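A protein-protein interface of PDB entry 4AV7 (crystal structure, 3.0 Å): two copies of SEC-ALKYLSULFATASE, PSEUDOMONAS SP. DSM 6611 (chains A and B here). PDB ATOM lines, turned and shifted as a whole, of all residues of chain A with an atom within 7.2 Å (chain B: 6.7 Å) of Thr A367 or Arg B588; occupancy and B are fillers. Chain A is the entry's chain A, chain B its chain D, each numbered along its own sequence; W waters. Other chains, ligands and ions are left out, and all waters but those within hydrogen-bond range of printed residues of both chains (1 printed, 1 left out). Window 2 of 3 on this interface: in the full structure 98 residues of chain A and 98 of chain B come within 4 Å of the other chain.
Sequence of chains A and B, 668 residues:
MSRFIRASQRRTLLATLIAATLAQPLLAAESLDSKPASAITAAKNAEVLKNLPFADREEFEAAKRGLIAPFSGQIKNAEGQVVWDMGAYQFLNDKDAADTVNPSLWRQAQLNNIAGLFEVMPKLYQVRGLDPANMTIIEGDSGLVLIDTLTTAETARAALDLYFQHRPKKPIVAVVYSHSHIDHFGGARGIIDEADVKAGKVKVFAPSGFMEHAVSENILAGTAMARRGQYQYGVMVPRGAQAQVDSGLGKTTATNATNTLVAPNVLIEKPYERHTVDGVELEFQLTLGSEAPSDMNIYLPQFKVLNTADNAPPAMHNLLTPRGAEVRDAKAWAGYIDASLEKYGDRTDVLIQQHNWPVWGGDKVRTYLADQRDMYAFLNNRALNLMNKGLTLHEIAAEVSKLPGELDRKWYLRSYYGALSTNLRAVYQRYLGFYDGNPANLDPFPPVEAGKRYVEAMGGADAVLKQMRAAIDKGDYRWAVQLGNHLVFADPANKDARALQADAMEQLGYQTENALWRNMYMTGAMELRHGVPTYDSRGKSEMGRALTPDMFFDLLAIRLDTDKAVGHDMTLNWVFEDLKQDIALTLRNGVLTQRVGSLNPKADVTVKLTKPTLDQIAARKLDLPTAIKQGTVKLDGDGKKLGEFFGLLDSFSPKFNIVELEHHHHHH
No position is printed for both chains.
Of the 11 pairs that touch across the chains among the printed residues, none has its exchanged pair printed and touching as well.
O of Asp A363 lies within hydrogen-bond range of OG1 of Thr A367, 3.3 Å away.
The side-chain carboxylate of Asp A371 is in salt-bridge range of the side-chain amino group of Lys A410 (3.6 Å).
OH of Tyr A412 is in hydrogen-bond range of OD2 of Asp A371 (2.6 Å).
The side-chain carboxylate of Asp A374 is in salt-bridge range of the guanidinium group of Arg A373 (3.0 Å).
OD1 of Asp B569 sits at hydrogen-bond distance from N of Asn B589 (3.1 Å).
The backbone NH of Thr B586 lies within hydrogen-bond range of the backbone carbonyl oxygen of Thr B593.
Among the printed residues, merely in contact across the chains: Ala A370 with Arg B588, Pro A404 with Asn B589, Leu A407 with Asn B589, Asp A374 with Val B591, Arg A373 with Arg B588, Asp A374 with Asn B589, Arg A373 with Thr B593 and Thr A367 with Arg B588.
Of the 20 printed residues of chain A, 8 touch a printed residue of chain B.
Hydrophobic or aromatic side chains of chain A that line the printed part of chain B: Ala A370, Pro A404 and Leu A407.
Hydrophobic or aromatic side chains of chain B within 4 Å of the printed part of chain A: Val B591.
Among the printed residues, Asp or Glu carboxylates within 4 Å of a Lys or Arg side-chain nitrogen of the other chain: Asp A371 with Arg B588 (2.7 Å) and Asp A374 with Arg B588 (2.8 Å).
Thr A367 touches just one residue of chain B: Arg B588.
Arg B588 touches just these residues of chain A: Thr A367 (3.9 Å), Ala A370 (3.1 Å), Asp A371 (2.7 Å), Arg A373 (3.6 Å) and Asp A374 (2.8 Å).
Of the printed residues of chain B, Glu A406 touches Asn B589 (3.1 Å).
Of the printed residues of chain B, Asp A371 touches Arg B588.
Printed residues of chain B within 4 Å of Pro A404: Asn B589 (3.4 Å).
Of the printed residues of chain B, Leu A407 touches Asn B589.
Of the printed residues of chain B, Asp A374 touches Arg B588 (2.8 Å), Asn B589 (3.6 Å) and Val B591 (3.5 Å).
Tyr A412 touches none of the printed residues of chain B.
His B568 touches none of the printed residues of chain A.
The nearest printed residue of chain B that does not touch Thr A367 is Asn B589 (7.8 Å).
The nearest printed residue of chain B that does not touch Asp A371 is Asn B589 (4.1 Å).
Water W1 lies within hydrogen-bond range of OG1 of Thr B593 (2.6 Å) and NH1 of Arg A373 (3.3 Å).
The guanidinium group of Arg B588 lies within salt-bridge range of the side-chain carboxylate of Asp A371.
The guanidinium group (NE) of Arg B588 lies within salt-bridge range of the side-chain carboxylate (OD2) of Asp A374 (2.8 Å).
The backbone NH (N) of Glu A406 is in hydrogen-bond range of the side-chain amide oxygen (OD1) of Asn B589 (3.1 Å).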
ATOM      1  N   LEU A 341      21.534  17.720   9.351  1.00  0.00           N
ATOM      2  CA  LEU A 341      22.520  17.247   8.389  1.00  0.00           C
ATOM      3  C   LEU A 341      23.924  17.236   8.983  1.00  0.00           C
ATOM      4  O   LEU A 341      24.664  16.254   8.807  1.00  0.00           O
ATOM      5  CB  LEU A 341      22.477  18.092   7.109  1.00  0.00           C
ATOM      6  CG  LEU A 341      23.522  17.745   6.038  1.00  0.00           C
ATOM      7  CD1 LEU A 341      23.424  16.285   5.577  1.00  0.00           C
ATOM      8  CD2 LEU A 341      23.437  18.734   4.879  1.00  0.00           C
ATOM      9  N   GLY A 361      19.942   4.537   3.803  1.00  0.00           N
ATOM     10  CA  GLY A 361      21.303   4.695   3.309  1.00  0.00           C
ATOM     11  C   GLY A 361      21.843   6.057   3.637  1.00  0.00           C
ATOM     12  O   GLY A 361      21.263   7.054   3.225  1.00  0.00           O
ATOM     13  N   GLY A 362      22.943   6.106   4.385  1.00  0.00           N
ATOM     14  CA  GLY A 362      23.550   7.389   4.800  1.00  0.00           C
ATOM     15  C   GLY A 362      23.780   8.411   3.690  1.00  0.00           C
ATOM     16  O   GLY A 362      23.422   9.588   3.820  1.00  0.00           O
ATOM     17  N   ASP A 363      24.373   7.946   2.593  1.00  0.00           N
ATOM     18  CA  ASP A 363      24.592   8.764   1.407  1.00  0.00           C
ATOM     19  C   ASP A 363      23.274   9.362   0.962  1.00  0.00           C
ATOM     20  O   ASP A 363      23.194  10.568   0.778  1.00  0.00           O
ATOM     21  CB  ASP A 363      25.236   7.934   0.288  1.00  0.00           C
ATOM     22  CG  ASP A 363      26.586   7.308   0.712  1.00  0.00           C
ATOM     23  OD1 ASP A 363      27.591   8.052   0.821  1.00  0.00           O
ATOM     24  OD2 ASP A 363      26.644   6.071   0.951  1.00  0.00           O
ATOM     25  N   LYS A 364      22.239   8.517   0.850  1.00  0.00           N
ATOM     26  CA  LYS A 364      20.884   8.925   0.469  1.00  0.00           C
ATOM     27  C   LYS A 364      20.242   9.909   1.433  1.00  0.00           C
ATOM     28  O   LYS A 364      19.626  10.871   0.979  1.00  0.00           O
ATOM     29  CB  LYS A 364      19.964   7.707   0.309  1.00  0.00           C
ATOM     30  CG  LYS A 364      20.011   7.043  -1.061  1.00  0.00           C
ATOM     31  CD  LYS A 364      18.971   5.938  -1.194  1.00  0.00           C
ATOM     32  CE  LYS A 364      18.711   5.632  -2.662  1.00  0.00           C
ATOM     33  NZ  LYS A 364      18.154   4.268  -2.857  1.00  0.00           N
ATOM     34  N   VAL A 365      20.353   9.671   2.744  1.00  0.00           N
ATOM     35  CA  VAL A 365      19.797  10.625   3.718  1.00  0.00           C
ATOM     36  C   VAL A 365      20.511  11.982   3.670  1.00  0.00           C
ATOM     37  O   VAL A 365      19.873  13.024   3.823  1.00  0.00           O
ATOM     38  CB  VAL A 365      19.661  10.108   5.198  1.00  0.00           C
ATOM     39  CG1 VAL A 365      18.923   8.780   5.283  1.00  0.00           C
ATOM     40  CG2 VAL A 365      20.994  10.012   5.905  1.00  0.00           C
ATOM     41  N   ARG A 366      21.824  11.978   3.443  1.00  0.00           N
ATOM     42  CA  ARG A 366      22.570  13.242   3.372  1.00  0.00           C
ATOM     43  C   ARG A 366      22.148  14.090   2.154  1.00  0.00           C
ATOM     44  O   ARG A 366      21.926  15.315   2.265  1.00  0.00           O
ATOM     45  CB  ARG A 366      24.085  12.995   3.416  1.00  0.00           C
ATOM     46  CG  ARG A 366      24.626  12.637   4.806  1.00  0.00           C
ATOM     47  CD  ARG A 366      26.143  12.391   4.800  1.00  0.00           C
ATOM     48  NE  ARG A 366      26.547  11.118   4.188  1.00  0.00           N
ATOM     49  CZ  ARG A 366      26.585   9.941   4.825  1.00  0.00           C
ATOM     50  NH1 ARG A 366      26.241   9.847   6.115  1.00  0.00           N
ATOM     51  NH2 ARG A 366      26.938   8.847   4.162  1.00  0.00           N
ATOM     52  N   THR A 367      22.005  13.418   1.013  1.00  0.00           N
ATOM     53  CA  THR A 367      21.463  14.027  -0.198  1.00  0.00           C
ATOM     54  C   THR A 367      20.056  14.555   0.058  1.00  0.00           C
ATOM     55  O   THR A 367      19.743  15.720  -0.202  1.00  0.00           O
ATOM     56  CB  THR A 367      21.487  13.024  -1.360  1.00  0.00           C
ATOM     57  OG1 THR A 367      22.859  12.736  -1.661  1.00  0.00           O
ATOM     58  CG2 THR A 367      20.839  13.601  -2.613  1.00  0.00           C
ATOM     59  N   TYR A 368      19.223  13.695   0.615  1.00  0.00           N
ATOM     60  CA  TYR A 368      17.867  14.057   0.988  1.00  0.00           C
ATOM     61  C   TYR A 368      17.828  15.344   1.801  1.00  0.00           C
ATOM     62  O   TYR A 368      17.157  16.289   1.398  1.00  0.00           O
ATOM     63  CB  TYR A 368      17.251  12.909   1.763  1.00  0.00           C
ATOM     64  CG  TYR A 368      15.795  13.027   2.025  1.00  0.00           C
ATOM     65  CD1 TYR A 368      14.850  12.681   1.054  1.00  0.00           C
ATOM     66  CD2 TYR A 368      15.351  13.428   3.263  1.00  0.00           C
ATOM     67  CE1 TYR A 368      13.492  12.770   1.322  1.00  0.00           C
ATOM     68  CE2 TYR A 368      13.993  13.528   3.550  1.00  0.00           C
ATOM     69  CZ  TYR A 368      13.065  13.203   2.582  1.00  0.00           C
ATOM     70  OH  TYR A 368      11.727  13.302   2.880  1.00  0.00           O
ATOM     71  N   LEU A 369      18.568  15.399   2.907  1.00  0.00           N
ATOM     72  CA  LEU A 369      18.493  16.555   3.811  1.00  0.00           C
ATOM     73  C   LEU A 369      19.115  17.795   3.183  1.00  0.00           C
ATOM     74  O   LEU A 369      18.625  18.920   3.381  1.00  0.00           O
ATOM     75  CB  LEU A 369      19.165  16.271   5.147  1.00  0.00           C
ATOM     76  CG  LEU A 369      18.631  15.171   6.041  1.00  0.00           C
ATOM     77  CD1 LEU A 369      19.671  14.935   7.113  1.00  0.00           C
ATOM     78  CD2 LEU A 369      17.343  15.602   6.681  1.00  0.00           C
ATOM     79  N   ALA A 370      20.197  17.584   2.428  1.00  0.00           N
ATOM     80  CA  ALA A 370      20.778  18.668   1.664  1.00  0.00           C
ATOM     81  C   ALA A 370      19.709  19.300   0.739  1.00  0.00           C
ATOM     82  O   ALA A 370      19.530  20.521   0.724  1.00  0.00           O
ATOM     83  CB  ALA A 370      21.959  18.162   0.879  1.00  0.00           C
ATOM     84  N   ASP A 371      18.979  18.461   0.009  1.00  0.00           N
ATOM     85  CA  ASP A 371      17.966  18.924  -0.908  1.00  0.00           C
ATOM     86  C   ASP A 371      16.822  19.622  -0.169  1.00  0.00           C
ATOM     87  O   ASP A 371      16.340  20.686  -0.577  1.00  0.00           O
ATOM     88  CB  ASP A 371      17.432  17.740  -1.709  1.00  0.00           C
ATOM     89  CG  ASP A 371      18.405  17.268  -2.787  1.00  0.00           C
ATOM     90  OD1 ASP A 371      18.989  18.131  -3.486  1.00  0.00           O
ATOM     91  OD2 ASP A 371      18.575  16.038  -2.954  1.00  0.00           O
ATOM     92  N   GLN A 372      16.381  19.027   0.926  1.00  0.00           N
ATOM     93  CA  GLN A 372      15.288  19.605   1.679  1.00  0.00           C
ATOM     94  C   GLN A 372      15.664  20.975   2.203  1.00  0.00           C
ATOM     95  O   GLN A 372      14.835  21.863   2.224  1.00  0.00           O
ATOM     96  CB  GLN A 372      14.894  18.683   2.810  1.00  0.00           C
ATOM     97  CG  GLN A 372      14.250  17.408   2.314  1.00  0.00           C
ATOM     98  CD  GLN A 372      12.738  17.507   2.303  1.00  0.00           C
ATOM     99  OE1 GLN A 372      12.145  18.465   2.835  1.00  0.00           O
ATOM    100  NE2 GLN A 372      12.102  16.511   1.711  1.00  0.00           N
ATOM    101  N   ARG A 373      16.923  21.149   2.600  1.00  0.00           N
ATOM    102  CA  ARG A 373      17.384  22.417   3.173  1.00  0.00           C
ATOM    103  C   ARG A 373      17.402  23.467   2.080  1.00  0.00           C
ATOM    104  O   ARG A 373      16.861  24.562   2.236  1.00  0.00           O
ATOM    105  CB  ARG A 373      18.767  22.261   3.795  1.00  0.00           C
ATOM    106  CG  ARG A 373      19.550  23.545   4.005  1.00  0.00           C
ATOM    107  CD  ARG A 373      21.039  23.245   3.938  1.00  0.00           C
ATOM    108  NE  ARG A 373      21.512  23.000   2.574  1.00  0.00           N
ATOM    109  CZ  ARG A 373      22.679  22.443   2.259  1.00  0.00           C
ATOM    110  NH1 ARG A 373      23.492  22.045   3.219  1.00  0.00           N
ATOM    111  NH2 ARG A 373      23.035  22.283   0.981  1.00  0.00           N
ATOM    112  N   ASP A 374      18.005  23.109   0.960  1.00  0.00           N
ATOM    113  CA  ASP A 374      18.055  23.989  -0.194  1.00  0.00           C
ATOM    114  C   ASP A 374      16.662  24.473  -0.591  1.00  0.00           C
ATOM    115  O   ASP A 374      16.503  25.628  -0.988  1.00  0.00           O
ATOM    116  CB  ASP A 374      18.713  23.271  -1.378  1.00  0.00           C
ATOM    117  CG  ASP A 374      20.201  23.063  -1.183  1.00  0.00           C
ATOM    118  OD1 ASP A 374      20.769  23.764  -0.322  1.00  0.00           O
ATOM    119  OD2 ASP A 374      20.794  22.223  -1.903  1.00  0.00           O
ATOM    120  N   PRO A 404      14.795  25.347  -8.282  1.00  0.00           N
ATOM    121  CA  PRO A 404      15.981  25.492  -9.146  1.00  0.00           C
ATOM    122  C   PRO A 404      16.845  24.246  -9.306  1.00  0.00           C
ATOM    123  O   PRO A 404      16.954  23.452  -8.377  1.00  0.00           O
ATOM    124  CB  PRO A 404      16.782  26.573  -8.451  1.00  0.00           C
ATOM    125  CG  PRO A 404      16.411  26.430  -7.029  1.00  0.00           C
ATOM    126  CD  PRO A 404      14.939  26.137  -7.054  1.00  0.00           C
ATOM    127  N   GLU A 406      18.769  20.856  -9.866  1.00  0.00           N
ATOM    128  CA  GLU A 406      18.422  19.466  -9.568  1.00  0.00           C
ATOM    129  C   GLU A 406      17.279  19.275  -8.603  1.00  0.00           C
ATOM    130  O   GLU A 406      16.746  18.164  -8.512  1.00  0.00           O
ATOM    131  CB  GLU A 406      19.633  18.696  -9.035  1.00  0.00           C
ATOM    132  CG  GLU A 406      20.696  18.429 -10.089  1.00  0.00           C
ATOM    133  CD  GLU A 406      20.100  17.946 -11.400  1.00  0.00           C
ATOM    134  OE1 GLU A 406      19.553  16.814 -11.430  1.00  0.00           O
ATOM    135  OE2 GLU A 406      20.174  18.708 -12.394  1.00  0.00           O
ATOM    136  N   LEU A 407      16.908  20.339  -7.884  1.00  0.00           N
ATOM    137  CA  LEU A 407      15.811  20.286  -6.925  1.00  0.00           C
ATOM    138  C   LEU A 407      14.472  20.018  -7.614  1.00  0.00           C
ATOM    139  O   LEU A 407      13.558  19.454  -6.995  1.00  0.00           O
ATOM    140  CB  LEU A 407      15.725  21.578  -6.108  1.00  0.00           C
ATOM    141  CG  LEU A 407      16.859  22.020  -5.179  1.00  0.00           C
ATOM    142  CD1 LEU A 407      16.426  23.291  -4.465  1.00  0.00           C
ATOM    143  CD2 LEU A 407      17.276  20.992  -4.135  1.00  0.00           C
ATOM    144  N   LYS A 410      13.531  15.910  -8.325  1.00  0.00           N
ATOM    145  CA  LYS A 410      13.405  14.930  -7.218  1.00  0.00           C
ATOM    146  C   LYS A 410      11.953  14.698  -6.842  1.00  0.00           C
ATOM    147  O   LYS A 410      11.205  15.651  -6.671  1.00  0.00           O
ATOM    148  CB  LYS A 410      14.181  15.357  -5.951  1.00  0.00           C
ATOM    149  CG  LYS A 410      15.583  15.913  -6.172  1.00  0.00           C
ATOM    150  CD  LYS A 410      16.618  14.814  -6.275  1.00  0.00           C
ATOM    151  CE  LYS A 410      17.997  15.407  -6.458  1.00  0.00           C
ATOM    152  NZ  LYS A 410      19.023  14.402  -6.091  1.00  0.00           N
ATOM    153  N   TYR A 412      10.775  13.593  -4.064  1.00  0.00           N
ATOM    154  CA  TYR A 412      10.520  13.997  -2.678  1.00  0.00           C
ATOM    155  C   TYR A 412      10.434  15.502  -2.416  1.00  0.00           C
ATOM    156  O   TYR A 412      10.174  15.907  -1.268  1.00  0.00           O
ATOM    157  CB  TYR A 412      11.516  13.352  -1.719  1.00  0.00           C
ATOM    158  CG  TYR A 412      12.973  13.555  -2.044  1.00  0.00           C
ATOM    159  CD1 TYR A 412      13.678  14.656  -1.557  1.00  0.00           C
ATOM    160  CD2 TYR A 412      13.662  12.615  -2.806  1.00  0.00           C
ATOM    161  CE1 TYR A 412      15.032  14.812  -1.841  1.00  0.00           C
ATOM    162  CE2 TYR A 412      15.008  12.762  -3.099  1.00  0.00           C
ATOM    163  CZ  TYR A 412      15.690  13.856  -2.613  1.00  0.00           C
ATOM    164  OH  TYR A 412      17.024  13.985  -2.925  1.00  0.00           O
ATOM    165  N   ALA B 565      23.025  31.698 -10.883  1.00  0.00           N
ATOM    166  CA  ALA B 565      23.857  30.880  -9.980  1.00  0.00           C
ATOM    167  C   ALA B 565      23.818  29.360 -10.175  1.00  0.00           C
ATOM    168  O   ALA B 565      24.712  28.651  -9.699  1.00  0.00           O
ATOM    169  CB  ALA B 565      23.561  31.222  -8.528  1.00  0.00           C
ATOM    170  N   HIS B 568      26.804  26.912 -11.223  1.00  0.00           N
ATOM    171  CA  HIS B 568      28.053  27.388 -10.599  1.00  0.00           C
ATOM    172  C   HIS B 568      28.244  26.939  -9.173  1.00  0.00           C
ATOM    173  O   HIS B 568      28.808  27.674  -8.362  1.00  0.00           O
ATOM    174  CB  HIS B 568      28.139  28.910 -10.661  1.00  0.00           C
ATOM    175  CG  HIS B 568      28.016  29.465 -12.049  1.00  0.00           C
ATOM    176  ND1 HIS B 568      29.085  29.843 -12.775  1.00  0.00           N
ATOM    177  CD2 HIS B 568      26.895  29.689 -12.848  1.00  0.00           C
ATOM    178  CE1 HIS B 568      28.673  30.296 -13.974  1.00  0.00           C
ATOM    179  NE2 HIS B 568      27.331  30.198 -14.017  1.00  0.00           N
ATOM    180  N   ASP B 569      27.786  25.726  -8.857  1.00  0.00           N
ATOM    181  CA  ASP B 569      27.889  25.167  -7.503  1.00  0.00           C
ATOM    182  C   ASP B 569      29.299  25.258  -6.944  1.00  0.00           C
ATOM    183  O   ASP B 569      30.267  24.955  -7.625  1.00  0.00           O
ATOM    184  CB  ASP B 569      27.382  23.726  -7.467  1.00  0.00           C
ATOM    185  CG  ASP B 569      25.871  23.639  -7.600  1.00  0.00           C
ATOM    186  OD1 ASP B 569      25.235  24.633  -8.025  1.00  0.00           O
ATOM    187  OD2 ASP B 569      25.302  22.570  -7.287  1.00  0.00           O
ATOM    188  N   MET B 570      29.399  25.706  -5.703  1.00  0.00           N
ATOM    189  CA  MET B 570      30.691  25.981  -5.098  1.00  0.00           C
ATOM    190  C   MET B 570      30.589  26.083  -3.569  1.00  0.00           C
ATOM    191  O   MET B 570      29.492  26.315  -3.022  1.00  0.00           O
ATOM    192  CB  MET B 570      31.282  27.266  -5.693  1.00  0.00           C
ATOM    193  CG  MET B 570      30.528  28.528  -5.327  1.00  0.00           C
ATOM    194  SD  MET B 570      31.318  30.023  -5.959  1.00  0.00           S
ATOM    195  CE  MET B 570      30.830  30.007  -7.680  1.00  0.00           C
ATOM    196  N   THR B 586      27.997  27.713   1.351  1.00  0.00           N
ATOM    197  CA  THR B 586      27.804  26.667   0.338  1.00  0.00           C
ATOM    198  C   THR B 586      26.711  27.066  -0.692  1.00  0.00           C
ATOM    199  O   THR B 586      25.562  27.415  -0.318  1.00  0.00           O
ATOM    200  CB  THR B 586      27.631  25.230   0.975  1.00  0.00           C
ATOM    201  OG1 THR B 586      26.611  24.490   0.289  1.00  0.00           O
ATOM    202  CG2 THR B 586      27.321  25.274   2.519  1.00  0.00           C
ATOM    203  N   LEU B 587      27.096  27.069  -1.971  1.00  0.00           N
ATOM    204  CA  LEU B 587      26.175  27.406  -3.056  1.00  0.00           C
ATOM    205  C   LEU B 587      25.831  26.154  -3.844  1.00  0.00           C
ATOM    206  O   LEU B 587      26.664  25.615  -4.571  1.00  0.00           O
ATOM    207  CB  LEU B 587      26.767  28.478  -3.977  1.00  0.00           C
ATOM    208  CG  LEU B 587      25.942  28.950  -5.182  1.00  0.00           C
ATOM    209  CD1 LEU B 587      24.731  29.725  -4.673  1.00  0.00           C
ATOM    210  CD2 LEU B 587      26.734  29.797  -6.176  1.00  0.00           C
ATOM    211  N   ARG B 588      24.600  25.689  -3.682  1.00  0.00           N
ATOM    212  CA  ARG B 588      24.154  24.433  -4.262  1.00  0.00           C
ATOM    213  C   ARG B 588      22.786  24.639  -4.911  1.00  0.00           C
ATOM    214  O   ARG B 588      21.830  25.074  -4.241  1.00  0.00           O
ATOM    215  CB  ARG B 588      24.046  23.376  -3.160  1.00  0.00           C
ATOM    216  CG  ARG B 588      23.962  21.927  -3.636  1.00  0.00           C
ATOM    217  CD  ARG B 588      24.184  20.944  -2.487  1.00  0.00           C
ATOM    218  NE  ARG B 588      22.929  20.351  -2.047  1.00  0.00           N
ATOM    219  CZ  ARG B 588      22.404  19.248  -2.569  1.00  0.00           C
ATOM    220  NH1 ARG B 588      23.028  18.619  -3.540  1.00  0.00           N
ATOM    221  NH2 ARG B 588      21.261  18.766  -2.124  1.00  0.00           N
ATOM    222  N   ASN B 589      22.702  24.333  -6.212  1.00  0.00           N
ATOM    223  CA  ASN B 589      21.465  24.481  -6.978  1.00  0.00           C
ATOM    224  C   ASN B 589      21.012  25.927  -6.991  1.00  0.00           C
ATOM    225  O   ASN B 589      19.816  26.205  -6.917  1.00  0.00           O
ATOM    226  CB  ASN B 589      20.326  23.630  -6.389  1.00  0.00           C
ATOM    227  CG  ASN B 589      20.557  22.135  -6.523  1.00  0.00           C
ATOM    228  OD1 ASN B 589      20.814  21.609  -7.610  1.00  0.00           O
ATOM    229  ND2 ASN B 589      20.438  21.434  -5.404  1.00  0.00           N
ATOM    230  N   GLY B 590      21.967  26.852  -7.059  1.00  0.00           N
ATOM    231  CA  GLY B 590      21.650  28.282  -7.075  1.00  0.00           C
ATOM    232  C   GLY B 590      21.097  28.842  -5.774  1.00  0.00           C
ATOM    233  O   GLY B 590      20.609  29.976  -5.746  1.00  0.00           O
ATOM    234  N   VAL B 591      21.179  28.051  -4.707  1.00  0.00           N
ATOM    235  CA  VAL B 591      20.726  28.445  -3.380  1.00  0.00           C
ATOM    236  C   VAL B 591      21.958  28.628  -2.503  1.00  0.00           C
ATOM    237  O   VAL B 591      22.850  27.767  -2.487  1.00  0.00           O
ATOM    238  CB  VAL B 591      19.852  27.345  -2.764  1.00  0.00           C
ATOM    239  CG1 VAL B 591      19.248  27.811  -1.463  1.00  0.00           C
ATOM    240  CG2 VAL B 591      18.745  26.954  -3.731  1.00  0.00           C
ATOM    241  N   LEU B 592      22.025  29.735  -1.773  1.00  0.00           N
ATOM    242  CA  LEU B 592      23.155  29.918  -0.846  1.00  0.00           C
ATOM    243  C   LEU B 592      22.804  29.620   0.613  1.00  0.00           C
ATOM    244  O   LEU B 592      21.855  30.172   1.174  1.00  0.00           O
ATOM    245  CB  LEU B 592      23.738  31.320  -0.974  1.00  0.00           C
ATOM    246  CG  LEU B 592      24.959  31.588  -0.127  1.00  0.00           C
ATOM    247  CD1 LEU B 592      26.210  31.042  -0.791  1.00  0.00           C
ATOM    248  CD2 LEU B 592      25.020  33.084   0.005  1.00  0.00           C
ATOM    249  N   THR B 593      23.588  28.757   1.234  1.00  0.00           N
ATOM    250  CA  THR B 593      23.384  28.431   2.649  1.00  0.00           C
ATOM    251  C   THR B 593      24.702  28.674   3.399  1.00  0.00           C
ATOM    252  O   THR B 593      25.766  28.639   2.777  1.00  0.00           O
ATOM    253  CB  THR B 593      22.858  26.975   2.781  1.00  0.00           C
ATOM    254  OG1 THR B 593      23.619  26.084   1.933  1.00  0.00           O
ATOM    255  CG2 THR B 593      21.394  26.905   2.351  1.00  0.00           C
HETATM  256  O   HOH W   1      24.517  25.017   4.176  1.00  0.00           O
